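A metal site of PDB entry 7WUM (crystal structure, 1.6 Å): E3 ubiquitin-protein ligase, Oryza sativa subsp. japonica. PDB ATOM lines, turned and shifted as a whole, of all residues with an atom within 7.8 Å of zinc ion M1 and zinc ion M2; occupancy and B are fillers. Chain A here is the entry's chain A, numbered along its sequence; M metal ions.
Of the 28 residues printed, 4 come within 4 Å of zinc ion M1.
The backbone NH of Cys 3 is in hydrogen-bond range of the backbone carbonyl oxygen of Cys 54, 2.9 Å away. SG of Cys 3 sits close to OG of Ser 5 (3.4 Å). N of Cys 54 sits close to SG of Cys 52. N of Arg 68 lies close to SG of Cys 66 (3.3 Å). The backbone NH (N) of Cys 52 is in hydrogen-bond range of the backbone carbonyl oxygen (O) of Ser 5 (2.9 Å).
Within 4 Å of zinc ion M2: Cys 3, Cys 28, Cys 31 and Cys 52.
Zinc ion M2 is bound by SG of Cys 3 (2.3 Å), SG of Cys 31 (2.3 Å), SG of Cys 52 (2.3 Å) and SG of Cys 28 (2.4 Å). Zinc ion M2 has four donor atoms within binding distance.
Zinc ion M1 is bound by ND1 of His 69 (2.0 Å), SG of Cys 66 (2.3 Å), SG of Cys 54 (2.3 Å) and SG of Cys 31 (2.4 Å). Zinc ion M1 has four donor atoms within binding distance.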
ATOM      1  N   ALA A   1     -17.905  -4.238  -6.036  1.00  0.00           N
ATOM      2  CA  ALA A   1     -19.165  -4.923  -6.392  1.00  0.00           C
ATOM      3  C   ALA A   1     -19.878  -4.204  -7.549  1.00  0.00           C
ATOM      4  O   ALA A   1     -20.122  -4.855  -8.560  1.00  0.00           O
ATOM      5  CB  ALA A   1     -20.046  -5.042  -5.182  1.00  0.00           C
ATOM      6  N   VAL A   2     -20.250  -2.937  -7.352  1.00  0.00           N
ATOM      7  CA  VAL A   2     -20.880  -2.132  -8.434  1.00  0.00           C
ATOM      8  C   VAL A   2     -19.939  -0.973  -8.746  1.00  0.00           C
ATOM      9  O   VAL A   2     -19.508  -0.294  -7.826  1.00  0.00           O
ATOM     10  CB  VAL A   2     -22.296  -1.626  -8.064  1.00  0.00           C
ATOM     11  CG1 VAL A   2     -22.822  -0.616  -9.075  1.00  0.00           C
ATOM     12  CG2 VAL A   2     -23.280  -2.769  -7.889  1.00  0.00           C
ATOM     13  N   CYS A   3     -19.648  -0.787 -10.022  1.00  0.00           N
ATOM     14  CA  CYS A   3     -18.721   0.279 -10.451  1.00  0.00           C
ATOM     15  C   CYS A   3     -19.166   1.620  -9.895  1.00  0.00           C
ATOM     16  O   CYS A   3     -20.335   1.971 -10.033  1.00  0.00           O
ATOM     17  CB  CYS A   3     -18.673   0.333 -11.965  1.00  0.00           C
ATOM     18  SG  CYS A   3     -17.413   1.472 -12.590  1.00  0.00           S
ATOM     19  N   GLY A   4     -18.229   2.332  -9.302  1.00  0.00           N
ATOM     20  CA  GLY A   4     -18.537   3.667  -8.820  1.00  0.00           C
ATOM     21  C   GLY A   4     -18.106   4.787  -9.745  1.00  0.00           C
ATOM     22  O   GLY A   4     -17.935   5.925  -9.297  1.00  0.00           O
ATOM     23  N   SER A   5     -17.925   4.503 -11.028  1.00  0.00           N
ATOM     24  CA  SER A   5     -17.564   5.539 -11.977  1.00  0.00           C
ATOM     25  C   SER A   5     -18.727   6.487 -12.207  1.00  0.00           C
ATOM     26  O   SER A   5     -19.888   6.074 -12.296  1.00  0.00           O
ATOM     27  CB  SER A   5     -17.107   4.921 -13.296  1.00  0.00           C
ATOM     28  OG  SER A   5     -15.810   4.357 -13.193  1.00  0.00           O
ATOM     29  N   VAL A   6     -18.417   7.776 -12.295  1.00  0.00           N
ATOM     30  CA  VAL A   6     -19.387   8.793 -12.656  1.00  0.00           C
ATOM     31  C   VAL A   6     -18.781   9.596 -13.793  1.00  0.00           C
ATOM     32  O   VAL A   6     -17.567   9.660 -13.944  1.00  0.00           O
ATOM     33  CB  VAL A   6     -19.746   9.690 -11.470  1.00  0.00           C
ATOM     34  CG1 VAL A   6     -20.356   8.877 -10.352  1.00  0.00           C
ATOM     35  CG2 VAL A   6     -18.513  10.406 -10.993  1.00  0.00           C
ATOM     36  N   TRP A   7     -19.647  10.157 -14.639  1.00  0.00           N
ATOM     37  CA  TRP A   7     -19.163  10.967 -15.742  1.00  0.00           C
ATOM     38  C   TRP A   7     -20.141  12.105 -16.024  1.00  0.00           C
ATOM     39  O   TRP A   7     -21.298  12.071 -15.592  1.00  0.00           O
ATOM     40  CB  TRP A   7     -18.899  10.123 -17.012  1.00  0.00           C
ATOM     41  CG  TRP A   7     -20.106   9.483 -17.576  1.00  0.00           C
ATOM     42  CD1 TRP A   7     -20.940  10.003 -18.521  1.00  0.00           C
ATOM     43  CD2 TRP A   7     -20.605   8.164 -17.285  1.00  0.00           C
ATOM     44  NE1 TRP A   7     -21.957   9.112 -18.802  1.00  0.00           N
ATOM     45  CE2 TRP A   7     -21.757   7.980 -18.059  1.00  0.00           C
ATOM     46  CE3 TRP A   7     -20.192   7.130 -16.442  1.00  0.00           C
ATOM     47  CZ2 TRP A   7     -22.509   6.812 -18.011  1.00  0.00           C
ATOM     48  CZ3 TRP A   7     -20.940   5.975 -16.397  1.00  0.00           C
ATOM     49  CH2 TRP A   7     -22.076   5.821 -17.181  1.00  0.00           C
ATOM     50  N   ALA A  26     -26.448   2.506 -18.645  1.00  0.00           N
ATOM     51  CA  ALA A  26     -25.190   2.726 -19.366  1.00  0.00           C
ATOM     52  C   ALA A  26     -24.055   2.251 -18.489  1.00  0.00           C
ATOM     53  O   ALA A  26     -24.160   2.188 -17.258  1.00  0.00           O
ATOM     54  CB  ALA A  26     -24.992   4.201 -19.723  1.00  0.00           C
ATOM     55  N   ILE A  27     -22.934   1.937 -19.141  1.00  0.00           N
ATOM     56  CA  ILE A  27     -21.724   1.568 -18.421  1.00  0.00           C
ATOM     57  C   ILE A  27     -20.563   2.407 -18.934  1.00  0.00           C
ATOM     58  O   ILE A  27     -20.554   2.869 -20.076  1.00  0.00           O
ATOM     59  CB  ILE A  27     -21.414   0.050 -18.507  1.00  0.00           C
ATOM     60  CG1 ILE A  27     -21.107  -0.404 -19.930  1.00  0.00           C
ATOM     61  CG2 ILE A  27     -22.549  -0.759 -17.844  1.00  0.00           C
ATOM     62  CD1 ILE A  27     -20.674  -1.856 -20.002  1.00  0.00           C
ATOM     63  N   CYS A  28     -19.577   2.617 -18.075  1.00  0.00           N
ATOM     64  CA  CYS A  28     -18.434   3.442 -18.422  1.00  0.00           C
ATOM     65  C   CYS A  28     -17.560   2.755 -19.461  1.00  0.00           C
ATOM     66  O   CYS A  28     -17.605   1.526 -19.636  1.00  0.00           O
ATOM     67  CB  CYS A  28     -17.632   3.792 -17.160  1.00  0.00           C
ATOM     68  SG  CYS A  28     -16.698   2.408 -16.398  1.00  0.00           S
ATOM     69  N   VAL A  29     -16.727   3.537 -20.136  1.00  0.00           N
ATOM     70  CA  VAL A  29     -15.875   2.975 -21.190  1.00  0.00           C
ATOM     71  C   VAL A  29     -14.984   1.849 -20.659  1.00  0.00           C
ATOM     72  O   VAL A  29     -14.966   0.771 -21.278  1.00  0.00           O
ATOM     73  CB  VAL A  29     -15.078   4.096 -21.886  1.00  0.00           C
ATOM     74  CG1 VAL A  29     -13.925   3.514 -22.690  1.00  0.00           C
ATOM     75  CG2 VAL A  29     -15.996   4.946 -22.762  1.00  0.00           C
ATOM     76  N   PRO A  30     -14.227   2.019 -19.566  1.00  0.00           N
ATOM     77  CA  PRO A  30     -13.419   0.884 -19.106  1.00  0.00           C
ATOM     78  C   PRO A  30     -14.228  -0.359 -18.790  1.00  0.00           C
ATOM     79  O   PRO A  30     -13.752  -1.460 -19.077  1.00  0.00           O
ATOM     80  CB  PRO A  30     -12.704   1.429 -17.870  1.00  0.00           C
ATOM     81  CG  PRO A  30     -12.824   2.893 -17.922  1.00  0.00           C
ATOM     82  CD  PRO A  30     -13.967   3.254 -18.806  1.00  0.00           C
ATOM     83  N   CYS A  31     -15.409  -0.222 -18.189  1.00  0.00           N
ATOM     84  CA  CYS A  31     -16.220  -1.414 -17.945  1.00  0.00           C
ATOM     85  C   CYS A  31     -16.648  -2.075 -19.246  1.00  0.00           C
ATOM     86  O   CYS A  31     -16.720  -3.315 -19.318  1.00  0.00           O
ATOM     87  CB  CYS A  31     -17.448  -1.070 -17.090  1.00  0.00           C
ATOM     88  SG  CYS A  31     -17.018  -0.894 -15.359  1.00  0.00           S
ATOM     89  N   PHE A  32     -16.959  -1.296 -20.264  1.00  0.00           N
ATOM     90  CA  PHE A  32     -17.294  -1.917 -21.535  1.00  0.00           C
ATOM     91  C   PHE A  32     -16.095  -2.633 -22.124  1.00  0.00           C
ATOM     92  O   PHE A  32     -16.205  -3.773 -22.599  1.00  0.00           O
ATOM     93  CB  PHE A  32     -17.835  -0.872 -22.520  1.00  0.00           C
ATOM     94  CG  PHE A  32     -18.203  -1.436 -23.849  1.00  0.00           C
ATOM     95  CD1 PHE A  32     -17.235  -1.621 -24.833  1.00  0.00           C
ATOM     96  CD2 PHE A  32     -19.494  -1.826 -24.091  1.00  0.00           C
ATOM     97  CE1 PHE A  32     -17.607  -2.173 -26.084  1.00  0.00           C
ATOM     98  CE2 PHE A  32     -19.853  -2.363 -25.328  1.00  0.00           C
ATOM     99  CZ  PHE A  32     -18.901  -2.556 -26.303  1.00  0.00           C
ATOM    100  N   ASN A  34     -13.577  -3.943 -20.699  1.00  0.00           N
ATOM    101  CA  ASN A  34     -13.188  -5.113 -19.940  1.00  0.00           C
ATOM    102  C   ASN A  34     -14.305  -6.143 -19.838  1.00  0.00           C
ATOM    103  O   ASN A  34     -14.207  -7.076 -19.025  1.00  0.00           O
ATOM    104  CB  ASN A  34     -12.699  -4.698 -18.551  1.00  0.00           C
ATOM    105  CG  ASN A  34     -11.330  -4.067 -18.583  1.00  0.00           C
ATOM    106  OD1 ASN A  34     -10.540  -4.318 -19.499  1.00  0.00           O
ATOM    107  ND2 ASN A  34     -11.038  -3.238 -17.592  1.00  0.00           N
ATOM    108  N   GLY A  35     -15.358  -6.003 -20.649  1.00  0.00           N
ATOM    109  CA  GLY A  35     -16.416  -6.977 -20.735  1.00  0.00           C
ATOM    110  C   GLY A  35     -16.528  -7.559 -22.137  1.00  0.00           C
ATOM    111  O   GLY A  35     -15.743  -7.252 -23.035  1.00  0.00           O
ATOM    112  N   CYS A  51     -24.021   7.488 -13.768  1.00  0.00           N
ATOM    113  CA  CYS A  51     -23.274   6.594 -12.907  1.00  0.00           C
ATOM    114  C   CYS A  51     -23.237   5.205 -13.534  1.00  0.00           C
ATOM    115  O   CYS A  51     -24.214   4.714 -14.200  1.00  0.00           O
ATOM    116  CB  CYS A  51     -23.887   6.502 -11.514  1.00  0.00           C
ATOM    117  SG  CYS A  51     -23.872   8.050 -10.586  1.00  0.00           S
ATOM    118  N   CYS A  52     -22.127   4.519 -13.409  1.00  0.00           N
ATOM    119  CA  CYS A  52     -21.983   3.254 -14.111  1.00  0.00           C
ATOM    120  C   CYS A  52     -22.883   2.183 -13.516  1.00  0.00           C
ATOM    121  O   CYS A  52     -23.012   2.066 -12.290  1.00  0.00           O
ATOM    122  CB  CYS A  52     -20.525   2.816 -14.097  1.00  0.00           C
ATOM    123  SG  CYS A  52     -20.223   1.342 -15.082  1.00  0.00           S
ATOM    124  N   ASP A  53     -23.509   1.400 -14.390  1.00  0.00           N
ATOM    125  CA  ASP A  53     -24.379   0.316 -13.964  1.00  0.00           C
ATOM    126  C   ASP A  53     -23.677  -1.034 -13.918  1.00  0.00           C
ATOM    127  O   ASP A  53     -24.329  -2.049 -13.623  1.00  0.00           O
ATOM    128  CB  ASP A  53     -25.596   0.218 -14.894  1.00  0.00           C
ATOM    129  CG  ASP A  53     -26.547   1.399 -14.728  1.00  0.00           C
ATOM    130  OD1 ASP A  53     -26.720   1.891 -13.605  1.00  0.00           O
ATOM    131  OD2 ASP A  53     -27.108   1.842 -15.747  1.00  0.00           O
ATOM    132  N   CYS A  54     -22.373  -1.084 -14.176  1.00  0.00           N
ATOM    133  CA  CYS A  54     -21.705  -2.374 -14.232  1.00  0.00           C
ATOM    134  C   CYS A  54     -21.656  -2.980 -12.834  1.00  0.00           C
ATOM    135  O   CYS A  54     -21.175  -2.347 -11.887  1.00  0.00           O
ATOM    136  CB  CYS A  54     -20.297  -2.223 -14.804  1.00  0.00           C
ATOM    137  SG  CYS A  54     -19.429  -3.770 -15.013  1.00  0.00           S
ATOM    138  N   GLY A  55     -22.153  -4.204 -12.710  1.00  0.00           N
ATOM    139  CA  GLY A  55     -22.199  -4.886 -11.426  1.00  0.00           C
ATOM    140  C   GLY A  55     -23.554  -4.857 -10.765  1.00  0.00           C
ATOM    141  O   GLY A  55     -23.783  -5.621  -9.819  1.00  0.00           O
ATOM    142  N   GLY A  64     -23.068  -9.232 -19.006  1.00  0.00           N
ATOM    143  CA  GLY A  64     -22.486  -8.009 -19.491  1.00  0.00           C
ATOM    144  C   GLY A  64     -21.621  -7.282 -18.500  1.00  0.00           C
ATOM    145  O   GLY A  64     -21.093  -6.221 -18.843  1.00  0.00           O
ATOM    146  N   PHE A  65     -21.445  -7.822 -17.291  1.00  0.00           N
ATOM    147  CA  PHE A  65     -20.527  -7.210 -16.335  1.00  0.00           C
ATOM    148  C   PHE A  65     -19.090  -7.376 -16.807  1.00  0.00           C
ATOM    149  O   PHE A  65     -18.709  -8.404 -17.369  1.00  0.00           O
ATOM    150  CB  PHE A  65     -20.641  -7.856 -14.957  1.00  0.00           C
ATOM    151  CG  PHE A  65     -21.964  -7.661 -14.263  1.00  0.00           C
ATOM    152  CD1 PHE A  65     -22.918  -6.778 -14.749  1.00  0.00           C
ATOM    153  CD2 PHE A  65     -22.231  -8.346 -13.075  1.00  0.00           C
ATOM    154  CE1 PHE A  65     -24.123  -6.603 -14.086  1.00  0.00           C
ATOM    155  CE2 PHE A  65     -23.432  -8.180 -12.413  1.00  0.00           C
ATOM    156  CZ  PHE A  65     -24.386  -7.317 -12.919  1.00  0.00           C
ATOM    157  N   CYS A  66     -18.267  -6.375 -16.526  1.00  0.00           N
ATOM    158  CA  CYS A  66     -16.852  -6.526 -16.813  1.00  0.00           C
ATOM    159  C   CYS A  66     -16.209  -7.522 -15.848  1.00  0.00           C
ATOM    160  O   CYS A  66     -16.821  -7.979 -14.880  1.00  0.00           O
ATOM    161  CB  CYS A  66     -16.149  -5.159 -16.761  1.00  0.00           C
ATOM    162  SG  CYS A  66     -15.683  -4.605 -15.111  1.00  0.00           S
ATOM    163  N   SER A  67     -14.961  -7.870 -16.146  1.00  0.00           N
ATOM    164  CA  SER A  67     -14.218  -8.817 -15.322  1.00  0.00           C
ATOM    165  C   SER A  67     -14.032  -8.347 -13.887  1.00  0.00           C
ATOM    166  O   SER A  67     -13.893  -9.171 -12.983  1.00  0.00           O
ATOM    167  CB  SER A  67     -12.866  -9.100 -15.997  1.00  0.00           C
ATOM    168  OG  SER A  67     -12.039  -7.948 -15.990  1.00  0.00           O
ATOM    169  N   ARG A  68     -14.077  -7.032 -13.658  1.00  0.00           N
ATOM    170  CA  ARG A  68     -13.714  -6.420 -12.388  1.00  0.00           C
ATOM    171  C   ARG A  68     -14.912  -6.168 -11.470  1.00  0.00           C
ATOM    172  O   ARG A  68     -14.716  -5.752 -10.333  1.00  0.00           O
ATOM    173  CB  ARG A  68     -12.962  -5.109 -12.651  1.00  0.00           C
ATOM    174  CG  ARG A  68     -11.760  -5.348 -13.572  1.00  0.00           C
ATOM    175  CD  ARG A  68     -10.831  -4.164 -13.860  1.00  0.00           C
ATOM    176  NE  ARG A  68     -10.293  -3.553 -12.659  1.00  0.00           N
ATOM    177  CZ  ARG A  68     -10.877  -2.562 -11.999  1.00  0.00           C
ATOM    178  NH1 ARG A  68     -11.950  -1.957 -12.465  1.00  0.00           N
ATOM    179  NH2 ARG A  68     -10.342  -2.146 -10.854  1.00  0.00           N
ATOM    180  N   HIS A  69     -16.141  -6.407 -11.947  1.00  0.00           N
ATOM    181  CA  HIS A  69     -17.337  -6.209 -11.146  1.00  0.00           C
ATOM    182  C   HIS A  69     -18.262  -7.397 -11.237  1.00  0.00           C
ATOM    183  O   HIS A  69     -19.370  -7.364 -10.692  1.00  0.00           O
ATOM    184  CB  HIS A  69     -18.069  -4.931 -11.580  1.00  0.00           C
ATOM    185  CG  HIS A  69     -17.224  -3.707 -11.445  1.00  0.00           C
ATOM    186  ND1 HIS A  69     -16.797  -2.969 -12.536  1.00  0.00           N
ATOM    187  CD2 HIS A  69     -16.647  -3.144 -10.358  1.00  0.00           C
ATOM    188  CE1 HIS A  69     -16.045  -1.971 -12.110  1.00  0.00           C
ATOM    189  NE2 HIS A  69     -15.916  -2.068 -10.796  1.00  0.00           N
ATOM    190  N   LYS A  70     -17.837  -8.459 -11.915  1.00  0.00           N
ATOM    191  CA  LYS A  70     -18.583  -9.709 -12.004  1.00  0.00           C
ATOM    192  C   LYS A  70     -18.685 -10.360 -10.632  1.00  0.00           C
ATOM    193  O   LYS A  70     -17.782 -11.093 -10.216  1.00  0.00           O
ATOM    194  CB  LYS A  70     -17.923 -10.651 -13.016  1.00  0.00           C
ATOM    195  CG  LYS A  70     -18.922 -11.302 -13.952  1.00  0.00           C
ATOM    196  CD  LYS A  70     -18.309 -11.612 -15.312  1.00  0.00           C
ATOM    197  CE  LYS A  70     -19.333 -12.228 -16.263  1.00  0.00           C
ATOM    198  NZ  LYS A  70     -19.606 -13.663 -15.986  1.00  0.00           N
HETATM  199 ZN    ZN M   1     -17.276  -3.079 -14.485  1.00  0.00          ZN
HETATM  200 ZN    ZN M   2     -17.898   1.164 -14.791  1.00  0.00          ZN
